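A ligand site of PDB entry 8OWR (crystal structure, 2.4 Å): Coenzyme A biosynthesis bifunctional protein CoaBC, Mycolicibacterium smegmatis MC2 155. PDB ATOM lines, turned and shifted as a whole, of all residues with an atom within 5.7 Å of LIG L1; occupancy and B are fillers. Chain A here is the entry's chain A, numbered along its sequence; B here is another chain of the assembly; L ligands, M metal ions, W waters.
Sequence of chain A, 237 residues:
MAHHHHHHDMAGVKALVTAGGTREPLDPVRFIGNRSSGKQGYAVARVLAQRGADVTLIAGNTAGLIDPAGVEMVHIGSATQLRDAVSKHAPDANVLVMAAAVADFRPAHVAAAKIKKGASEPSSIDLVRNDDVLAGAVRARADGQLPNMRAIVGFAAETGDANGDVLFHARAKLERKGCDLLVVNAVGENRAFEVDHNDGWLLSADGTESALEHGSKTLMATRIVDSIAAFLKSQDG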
ATOM      1  N   GLY A  20      -9.732   3.949   6.426  1.00  0.00           N
ATOM      2  CA  GLY A  20      -9.511   3.464   5.080  1.00  0.00           C
ATOM      3  C   GLY A  20     -10.825   3.252   4.352  1.00  0.00           C
ATOM      4  O   GLY A  20     -11.911   3.528   4.853  1.00  0.00           O
ATOM      5  N   SER A  36     -10.063   7.022  -0.666  1.00  0.00           N
ATOM      6  CA  SER A  36      -9.775   7.420   0.707  1.00  0.00           C
ATOM      7  C   SER A  36      -8.418   6.976   1.192  1.00  0.00           C
ATOM      8  O   SER A  36      -8.009   5.850   0.947  1.00  0.00           O
ATOM      9  CB  SER A  36     -10.857   6.967   1.659  1.00  0.00           C
ATOM     10  OG  SER A  36     -10.308   6.368   2.804  1.00  0.00           O
ATOM     11  N   SER A  37      -7.712   7.865   1.858  1.00  0.00           N
ATOM     12  CA  SER A  37      -6.365   7.533   2.314  1.00  0.00           C
ATOM     13  C   SER A  37      -6.343   6.834   3.654  1.00  0.00           C
ATOM     14  O   SER A  37      -5.392   6.083   3.940  1.00  0.00           O
ATOM     15  CB  SER A  37      -5.522   8.805   2.391  1.00  0.00           C
ATOM     16  OG  SER A  37      -5.966   9.611   3.461  1.00  0.00           O
ATOM     17  N   GLY A  38      -7.332   7.086   4.505  1.00  0.00           N
ATOM     18  CA  GLY A  38      -7.306   6.557   5.863  1.00  0.00           C
ATOM     19  C   GLY A  38      -6.451   7.346   6.824  1.00  0.00           C
ATOM     20  O   GLY A  38      -6.371   6.965   7.998  1.00  0.00           O
ATOM     21  N   LYS A  39      -5.814   8.429   6.379  1.00  0.00           N
ATOM     22  CA  LYS A  39      -4.821   9.099   7.193  1.00  0.00           C
ATOM     23  C   LYS A  39      -5.450   9.757   8.424  1.00  0.00           C
ATOM     24  O   LYS A  39      -4.858   9.740   9.519  1.00  0.00           O
ATOM     25  CB  LYS A  39      -4.085  10.157   6.359  1.00  0.00           C
ATOM     26  CG  LYS A  39      -3.070   9.586   5.373  1.00  0.00           C
ATOM     27  CD  LYS A  39      -2.329  10.677   4.603  1.00  0.00           C
ATOM     28  N   GLN A  40      -6.641  10.327   8.265  1.00  0.00           N
ATOM     29  CA  GLN A  40      -7.264  11.008   9.386  1.00  0.00           C
ATOM     30  C   GLN A  40      -7.775   9.997  10.429  1.00  0.00           C
ATOM     31  O   GLN A  40      -7.750  10.281  11.624  1.00  0.00           O
ATOM     32  CB  GLN A  40      -8.377  11.921   8.875  1.00  0.00           C
ATOM     33  CG  GLN A  40      -8.793  13.042   9.839  1.00  0.00           C
ATOM     34  CD  GLN A  40      -7.643  13.994  10.192  1.00  0.00           C
ATOM     35  OE1 GLN A  40      -7.210  14.795   9.354  1.00  0.00           O
ATOM     36  NE2 GLN A  40      -7.165  13.938  11.431  1.00  0.00           N
ATOM     37  N   GLY A  41      -8.227   8.825   9.986  1.00  0.00           N
ATOM     38  CA  GLY A  41      -8.609   7.796  10.947  1.00  0.00           C
ATOM     39  C   GLY A  41      -7.413   7.250  11.702  1.00  0.00           C
ATOM     40  O   GLY A  41      -7.457   7.101  12.921  1.00  0.00           O
ATOM     41  N   TYR A  42      -6.310   6.988  10.987  1.00  0.00           N
ATOM     42  CA  TYR A  42      -5.076   6.605  11.648  1.00  0.00           C
ATOM     43  C   TYR A  42      -4.626   7.681  12.625  1.00  0.00           C
ATOM     44  O   TYR A  42      -4.203   7.361  13.739  1.00  0.00           O
ATOM     45  CB  TYR A  42      -3.978   6.347  10.615  1.00  0.00           C
ATOM     46  CG  TYR A  42      -3.978   4.940  10.058  1.00  0.00           C
ATOM     47  CD1 TYR A  42      -5.140   4.393   9.527  1.00  0.00           C
ATOM     48  CD2 TYR A  42      -2.826   4.158  10.063  1.00  0.00           C
ATOM     49  CE1 TYR A  42      -5.138   3.121   9.013  1.00  0.00           C
ATOM     50  CE2 TYR A  42      -2.818   2.880   9.564  1.00  0.00           C
ATOM     51  CZ  TYR A  42      -3.976   2.364   9.031  1.00  0.00           C
ATOM     52  OH  TYR A  42      -3.983   1.093   8.514  1.00  0.00           O
ATOM     53  N   ALA A  99     -14.442   6.198  11.045  1.00  0.00           N
ATOM     54  CA  ALA A  99     -13.730   7.036  10.074  1.00  0.00           C
ATOM     55  C   ALA A  99     -13.601   6.395   8.692  1.00  0.00           C
ATOM     56  O   ALA A  99     -13.088   7.026   7.771  1.00  0.00           O
ATOM     57  CB  ALA A  99     -12.343   7.419  10.602  1.00  0.00           C
ATOM     58  N   ALA A 100     -14.032   5.159   8.530  1.00  0.00           N
ATOM     59  CA  ALA A 100     -13.880   4.478   7.261  1.00  0.00           C
ATOM     60  C   ALA A 100     -14.903   4.998   6.249  1.00  0.00           C
ATOM     61  O   ALA A 100     -16.008   5.443   6.604  1.00  0.00           O
ATOM     62  CB  ALA A 100     -14.040   2.978   7.442  1.00  0.00           C
ATOM     63  N   ALA A 101     -14.505   4.981   4.983  1.00  0.00           N
ATOM     64  CA  ALA A 101     -15.455   5.182   3.892  1.00  0.00           C
ATOM     65  C   ALA A 101     -16.034   3.814   3.546  1.00  0.00           C
ATOM     66  O   ALA A 101     -15.496   3.094   2.710  1.00  0.00           O
ATOM     67  CB  ALA A 101     -14.799   5.840   2.694  1.00  0.00           C
ATOM     68  N   VAL A 102     -17.132   3.444   4.211  1.00  0.00           N
ATOM     69  CA  VAL A 102     -17.760   2.143   4.013  1.00  0.00           C
ATOM     70  C   VAL A 102     -18.613   2.180   2.750  1.00  0.00           C
ATOM     71  O   VAL A 102     -19.461   3.050   2.586  1.00  0.00           O
ATOM     72  CB  VAL A 102     -18.608   1.725   5.236  1.00  0.00           C
ATOM     73  CG1 VAL A 102     -19.039   0.280   5.130  1.00  0.00           C
ATOM     74  CG2 VAL A 102     -17.842   1.914   6.557  1.00  0.00           C
ATOM     75  N   PHE A 155     -18.071  10.173  10.548  1.00  0.00           N
ATOM     76  CA  PHE A 155     -17.372  11.070   9.639  1.00  0.00           C
ATOM     77  C   PHE A 155     -18.228  11.313   8.398  1.00  0.00           C
ATOM     78  O   PHE A 155     -19.063  10.488   8.029  1.00  0.00           O
ATOM     79  CB  PHE A 155     -16.018  10.522   9.192  1.00  0.00           C
ATOM     80  CG  PHE A 155     -14.931  10.752  10.177  1.00  0.00           C
ATOM     81  CD1 PHE A 155     -15.009  10.233  11.469  1.00  0.00           C
ATOM     82  CD2 PHE A 155     -13.800  11.474   9.806  1.00  0.00           C
ATOM     83  CE1 PHE A 155     -13.983  10.436  12.371  1.00  0.00           C
ATOM     84  CE2 PHE A 155     -12.776  11.680  10.717  1.00  0.00           C
ATOM     85  CZ  PHE A 155     -12.862  11.159  11.997  1.00  0.00           C
ATOM     86  N   ALA A 156     -18.044  12.471   7.778  1.00  0.00           N
ATOM     87  CA  ALA A 156     -18.744  12.773   6.531  1.00  0.00           C
ATOM     88  C   ALA A 156     -17.863  13.684   5.686  1.00  0.00           C
ATOM     89  O   ALA A 156     -17.248  14.612   6.221  1.00  0.00           O
ATOM     90  CB  ALA A 156     -20.111  13.442   6.764  1.00  0.00           C
ATOM     91  N   ALA A 157     -17.821  13.422   4.386  1.00  0.00           N
ATOM     92  CA  ALA A 157     -17.241  14.365   3.437  1.00  0.00           C
ATOM     93  C   ALA A 157     -18.412  14.988   2.699  1.00  0.00           C
ATOM     94  O   ALA A 157     -19.052  14.330   1.873  1.00  0.00           O
ATOM     95  CB  ALA A 157     -16.278  13.683   2.473  1.00  0.00           C
ATOM     96  N   VAL A 183     -17.860  14.442  12.536  1.00  0.00           N
ATOM     97  CA  VAL A 183     -16.688  15.174  12.070  1.00  0.00           C
ATOM     98  C   VAL A 183     -16.890  15.379  10.582  1.00  0.00           C
ATOM     99  O   VAL A 183     -16.952  14.412   9.818  1.00  0.00           O
ATOM    100  CB  VAL A 183     -15.383  14.423  12.371  1.00  0.00           C
ATOM    101  CG1 VAL A 183     -14.163  15.249  11.956  1.00  0.00           C
ATOM    102  CG2 VAL A 183     -15.296  14.047  13.858  1.00  0.00           C
ATOM    103  N   VAL A 184     -17.003  16.629  10.168  1.00  0.00           N
ATOM    104  CA  VAL A 184     -17.353  16.980   8.802  1.00  0.00           C
ATOM    105  C   VAL A 184     -16.110  17.511   8.106  1.00  0.00           C
ATOM    106  O   VAL A 184     -15.404  18.369   8.628  1.00  0.00           O
ATOM    107  CB  VAL A 184     -18.480  18.035   8.786  1.00  0.00           C
ATOM    108  CG1 VAL A 184     -18.815  18.410   7.347  1.00  0.00           C
ATOM    109  CG2 VAL A 184     -19.706  17.507   9.531  1.00  0.00           C
ATOM    110  N   ASN A 185     -15.835  16.968   6.933  1.00  0.00           N
ATOM    111  CA  ASN A 185     -14.808  17.505   6.054  1.00  0.00           C
ATOM    112  C   ASN A 185     -15.552  18.188   4.922  1.00  0.00           C
ATOM    113  O   ASN A 185     -16.248  17.525   4.138  1.00  0.00           O
ATOM    114  CB  ASN A 185     -13.846  16.437   5.549  1.00  0.00           C
ATOM    115  CG  ASN A 185     -12.782  17.003   4.599  1.00  0.00           C
ATOM    116  OD1 ASN A 185     -12.262  18.091   4.827  1.00  0.00           O
ATOM    117  ND2 ASN A 185     -12.455  16.255   3.552  1.00  0.00           N
ATOM    118  N   LEU A 212     -13.512  23.376  12.346  1.00  0.00           N
ATOM    119  CA  LEU A 212     -12.280  22.618  12.407  1.00  0.00           C
ATOM    120  C   LEU A 212     -11.299  23.278  11.450  1.00  0.00           C
ATOM    121  O   LEU A 212     -11.409  23.116  10.235  1.00  0.00           O
ATOM    122  CB  LEU A 212     -12.569  21.154  12.044  1.00  0.00           C
ATOM    123  CG  LEU A 212     -11.701  19.984  12.500  1.00  0.00           C
ATOM    124  CD1 LEU A 212     -11.334  20.025  13.993  1.00  0.00           C
ATOM    125  CD2 LEU A 212     -12.537  18.791  12.200  1.00  0.00           C
ATOM    126  N   LYS A 217      -2.703  16.646   9.805  1.00  0.00           N
ATOM    127  CA  LYS A 217      -3.560  15.541  10.202  1.00  0.00           C
ATOM    128  C   LYS A 217      -3.486  15.273  11.705  1.00  0.00           C
ATOM    129  O   LYS A 217      -4.475  14.842  12.303  1.00  0.00           O
ATOM    130  CB  LYS A 217      -3.182  14.286   9.410  1.00  0.00           C
ATOM    131  CG  LYS A 217      -3.515  14.332   7.910  1.00  0.00           C
ATOM    132  CD  LYS A 217      -4.956  14.000   7.605  1.00  0.00           C
ATOM    133  CE  LYS A 217      -5.382  14.472   6.222  1.00  0.00           C
ATOM    134  NZ  LYS A 217      -6.700  15.198   6.287  1.00  0.00           N
ATOM    135  N   MET A 220      -5.513  18.290  13.731  1.00  0.00           N
ATOM    136  CA  MET A 220      -6.942  18.122  13.582  1.00  0.00           C
ATOM    137  C   MET A 220      -7.435  16.896  14.352  1.00  0.00           C
ATOM    138  O   MET A 220      -8.553  16.897  14.884  1.00  0.00           O
ATOM    139  CB  MET A 220      -7.289  18.015  12.101  1.00  0.00           C
ATOM    140  CG  MET A 220      -7.215  19.337  11.324  1.00  0.00           C
ATOM    141  SD  MET A 220      -7.617  19.184   9.567  1.00  0.00           S
ATOM    142  CE  MET A 220      -6.469  17.922   9.039  1.00  0.00           C
ATOM    143  N   ILE A 224     -10.259  16.611  17.337  1.00  0.00           N
ATOM    144  CA  ILE A 224     -11.285  15.583  17.330  1.00  0.00           C
ATOM    145  C   ILE A 224     -11.297  14.821  18.655  1.00  0.00           C
ATOM    146  O   ILE A 224     -12.358  14.568  19.246  1.00  0.00           O
ATOM    147  CB  ILE A 224     -11.114  14.619  16.133  1.00  0.00           C
ATOM    148  CG1 ILE A 224     -11.438  15.333  14.818  1.00  0.00           C
ATOM    149  CG2 ILE A 224     -12.006  13.391  16.293  1.00  0.00           C
ATOM    150  CD1 ILE A 224     -10.887  14.649  13.589  1.00  0.00           C
ATOM    151  N   VAL B  29     -14.923   9.795  -6.632  1.00  0.00           N
ATOM    152  CA  VAL B  29     -14.433   9.122  -5.426  1.00  0.00           C
ATOM    153  C   VAL B  29     -14.305   7.610  -5.624  1.00  0.00           C
ATOM    154  O   VAL B  29     -13.355   6.997  -5.117  1.00  0.00           O
ATOM    155  CB  VAL B  29     -15.369   9.451  -4.246  1.00  0.00           C
ATOM    156  CG1 VAL B  29     -15.320   8.365  -3.169  1.00  0.00           C
ATOM    157  CG2 VAL B  29     -15.021  10.805  -3.675  1.00  0.00           C
HETATM  158  C1  LIG L   1     -15.215   9.579   4.329  1.00  0.00           C
HETATM  159  C2  LIG L   1     -17.643   9.014   3.122  1.00  0.00           C
HETATM  160  C3  LIG L   1     -15.377   9.721   2.958  1.00  0.00           C
HETATM  161  C4  LIG L   1     -12.384  14.896   8.768  1.00  0.00           C
HETATM  162  C5  LIG L   1     -10.724  16.622   8.731  1.00  0.00           C
HETATM  163  C6  LIG L   1     -10.839  15.045   6.938  1.00  0.00           C
HETATM  164  C7  LIG L   1     -11.679  12.167   6.390  1.00  0.00           C
HETATM  165  C8  LIG L   1     -12.512  13.207   6.841  1.00  0.00           C
HETATM  166  C9  LIG L   1     -13.880  13.170   6.583  1.00  0.00           C
HETATM  167  C10 LIG L   1     -14.432  12.094   5.893  1.00  0.00           C
HETATM  168  C11 LIG L   1     -13.594  11.048   5.458  1.00  0.00           C
HETATM  169  C12 LIG L   1     -12.231  11.078   5.695  1.00  0.00           C
HETATM  170  C13 LIG L   1     -11.712   9.902   5.119  1.00  0.00           C
HETATM  171  C14 LIG L   1     -12.799   9.233   4.571  1.00  0.00           C
HETATM  172  C15 LIG L   1     -16.271   9.168   5.113  1.00  0.00           C
HETATM  173  C16 LIG L   1     -17.484   8.876   4.503  1.00  0.00           C
HETATM  174  C17 LIG L   1     -16.586   9.448   2.341  1.00  0.00           C
HETATM  175  C18 LIG L   1     -10.254   9.412   5.101  1.00  0.00           C
HETATM  176  C19 LIG L   1      -9.278   9.917   6.139  1.00  0.00           C
HETATM  177  C20 LIG L   1     -11.905  14.405   7.571  1.00  0.00           C
HETATM  178  C21 LIG L   1     -11.787  16.000   9.357  1.00  0.00           C
HETATM  179  C22 LIG L   1     -10.246  16.156   7.511  1.00  0.00           C
HETATM  180  N1  LIG L   1     -13.888   9.924   4.801  1.00  0.00           N
HETATM  181  O1  LIG L   1     -16.731   9.602   0.956  1.00  0.00           O
HETATM  182  O2  LIG L   1     -18.850   8.737   2.496  1.00  0.00           O
HETATM  183  O3  LIG L   1      -8.538  10.898   5.866  1.00  0.00           O
HETATM  184  O4  LIG L   1      -9.220   9.354   7.250  1.00  0.00           O
HETATM  185  O5  LIG L   1      -9.859   8.638   4.296  1.00  0.00           O
HETATM  186  O6  LIG L   1      -9.167  16.778   6.867  1.00  0.00           O
HETATM  187  N1  LG2 L   2     -20.754   4.274   7.399  1.00  0.00           N
HETATM  188  C1  LG2 L   2     -21.056   3.073   7.973  1.00  0.00           C
HETATM  189  N2  LG2 L   2     -21.705   2.121   7.204  1.00  0.00           N
HETATM  190  C2  LG2 L   2     -21.994   2.386   5.880  1.00  0.00           C
HETATM  191  C3  LG2 L   2     -21.726   3.626   5.358  1.00  0.00           C
HETATM  192  C4  LG2 L   2     -21.386   4.620   6.252  1.00  0.00           C
HETATM  193  O1  LG2 L   2     -20.766   2.849   9.145  1.00  0.00           O
HETATM  194  N3  LG2 L   2     -22.534   1.461   5.105  1.00  0.00           N
HETATM  195  C5  LG2 L   2     -20.300   5.351   8.264  1.00  0.00           C
HETATM  196  C6  LG2 L   2     -19.057   6.026   7.719  1.00  0.00           C
HETATM  197  O2  LG2 L   2     -17.877   5.452   8.213  1.00  0.00           O
HETATM  198  C7  LG2 L   2     -19.249   7.446   8.220  1.00  0.00           C
HETATM  199  C8  LG2 L   2     -20.746   7.627   8.350  1.00  0.00           C
HETATM  200  O3  LG2 L   2     -21.298   6.345   8.253  1.00  0.00           O
HETATM  201  O4  LG2 L   2     -18.791   7.596   9.532  1.00  0.00           O
HETATM  202  C9  LG2 L   2     -21.387   8.527   7.308  1.00  0.00           C
HETATM  203  O5  LG2 L   2     -20.799   8.336   6.044  1.00  0.00           O
HETATM  204  P1  LG2 L   2     -21.569   8.936   4.761  1.00  0.00           P
HETATM  205  O6  LG2 L   2     -21.044   8.194   3.562  1.00  0.00           O
HETATM  206  O7  LG2 L   2     -21.357  10.426   4.644  1.00  0.00           O
HETATM  207  O8  LG2 L   2     -23.130   8.623   5.077  1.00  0.00           O
HETATM  208  P2  LG2 L   2     -24.191   8.211   3.942  1.00  0.00           P
HETATM  209  O9  LG2 L   2     -25.543   7.867   4.518  1.00  0.00           O
HETATM  210  O10 LG2 L   2     -23.669   7.032   3.155  1.00  0.00           O
HETATM  211  O11 LG2 L   2     -24.266   9.595   3.122  1.00  0.00           O
HETATM  212  P3  LG2 L   2     -24.434   9.721   1.531  1.00  0.00           P
HETATM  213  O12 LG2 L   2     -25.528   8.759   1.130  1.00  0.00           O
HETATM  214  O13 LG2 L   2     -24.739  11.163   1.162  1.00  0.00           O
HETATM  215  O14 LG2 L   2     -23.179   9.291   0.839  1.00  0.00           O
HETATM  216 CA    CA M   1     -21.826   7.136   1.536  1.00  0.00          CA
HETATM  217  O   HOH W   1     -19.643  11.713   3.308  1.00  0.00           O
HETATM  218  O   HOH W   2     -10.300   6.736   7.458  1.00  0.00           O
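The side-chain hydroxyl (OG) of Ser 36 is in hydrogen-bond range of an oxygen (O5) of LIG L1 (2.8 Å).
The backbone NH of Gly 38 sits at hydrogen-bond distance from an oxygen (O5) of LIG L1, at 3.0 Å.
The backbone carbonyl oxygen of Ala 100 lies within hydrogen-bond range of an oxygen (O2) of LG2 L2, 2.5 Å away.
NZ of Lys 217 is in hydrogen-bond range of O6 of LIG L1, 3.0 Å away.
O of Phe 155 sits close to O4 of LG2 L2, at 3.3 Å.
An oxygen (O4) of LIG L1 lies within hydrogen-bond range of the backbone NH (N) of Gln 40 (2.9 Å).
The backbone NH (N) of Phe 155 sits at hydrogen-bond distance from an oxygen (O4) of LG2 L2 (2.9 Å).
The backbone NH (N) of Ser 37 lies within hydrogen-bond range of an oxygen (O5) of LIG L1 (3.3 Å).
The backbone NH (N) of Gly 41 lies within hydrogen-bond range of an oxygen (O4) of LIG L1, 3.0 Å away.
An oxygen (O6) of LG2 L2 sits close to an oxygen (O2) of LIG L1 (2.5 Å).
The backbone NH (N) of Lys 39 lies within hydrogen-bond range of the side-chain hydroxyl (OG) of Ser 37, 3.2 Å away.
O of Lys 217 sits at hydrogen-bond distance from NE2 of Gln 40 (3.0 Å).
The backbone NH (N) of Ala 101 sits at hydrogen-bond distance from the backbone carbonyl oxygen (O) of Gly 20 (3.0 Å).
The backbone carbonyl oxygen (O) of Val 183 lies within hydrogen-bond range of the backbone NH (N) of Ala 156 (3.0 Å).
The backbone carbonyl oxygen of Ala 156 sits at hydrogen-bond distance from the backbone NH of Asn 185 (2.8 Å).
Merely in contact with LIG L1: Asn 185 (3.4 Å), Val 183 (3.6 Å), Lys 39 (3.6 Å), Phe 155 (3.6 Å), Met 220 (3.6 Å), Ala 156 (3.7 Å), Ala 99 (3.9 Å), Ala 101 (3.9 Å) and Ala 157 (3.9 Å).
Hydrophobic or aromatic side chains within 4 Å of LIG L1: Ala 101, Phe 155, Val 183 and Met 220.
15 residues have an atom within 4 Å of LIG L1: Ser 36, Ser 37, Gly 38, Lys 39, Gln 40, Gly 41, Ala 99, Ala 101, Phe 155, Ala 156, Ala 157, Val 183, Asn 185, Lys 217 and Met 220.
Water W2 lies within hydrogen-bond range of the backbone carbonyl oxygen of Ala 99 (2.8 Å), an oxygen (O4) of LIG L1 (2.8 Å) and the backbone NH of Gly 20 (3.0 Å).
Water W1 lies within hydrogen-bond range of an oxygen (O7) of LG2 L2 (2.5 Å), the backbone NH (N) of Ala 157 (2.7 Å) and an oxygen (O2) of LIG L1 (3.2 Å).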
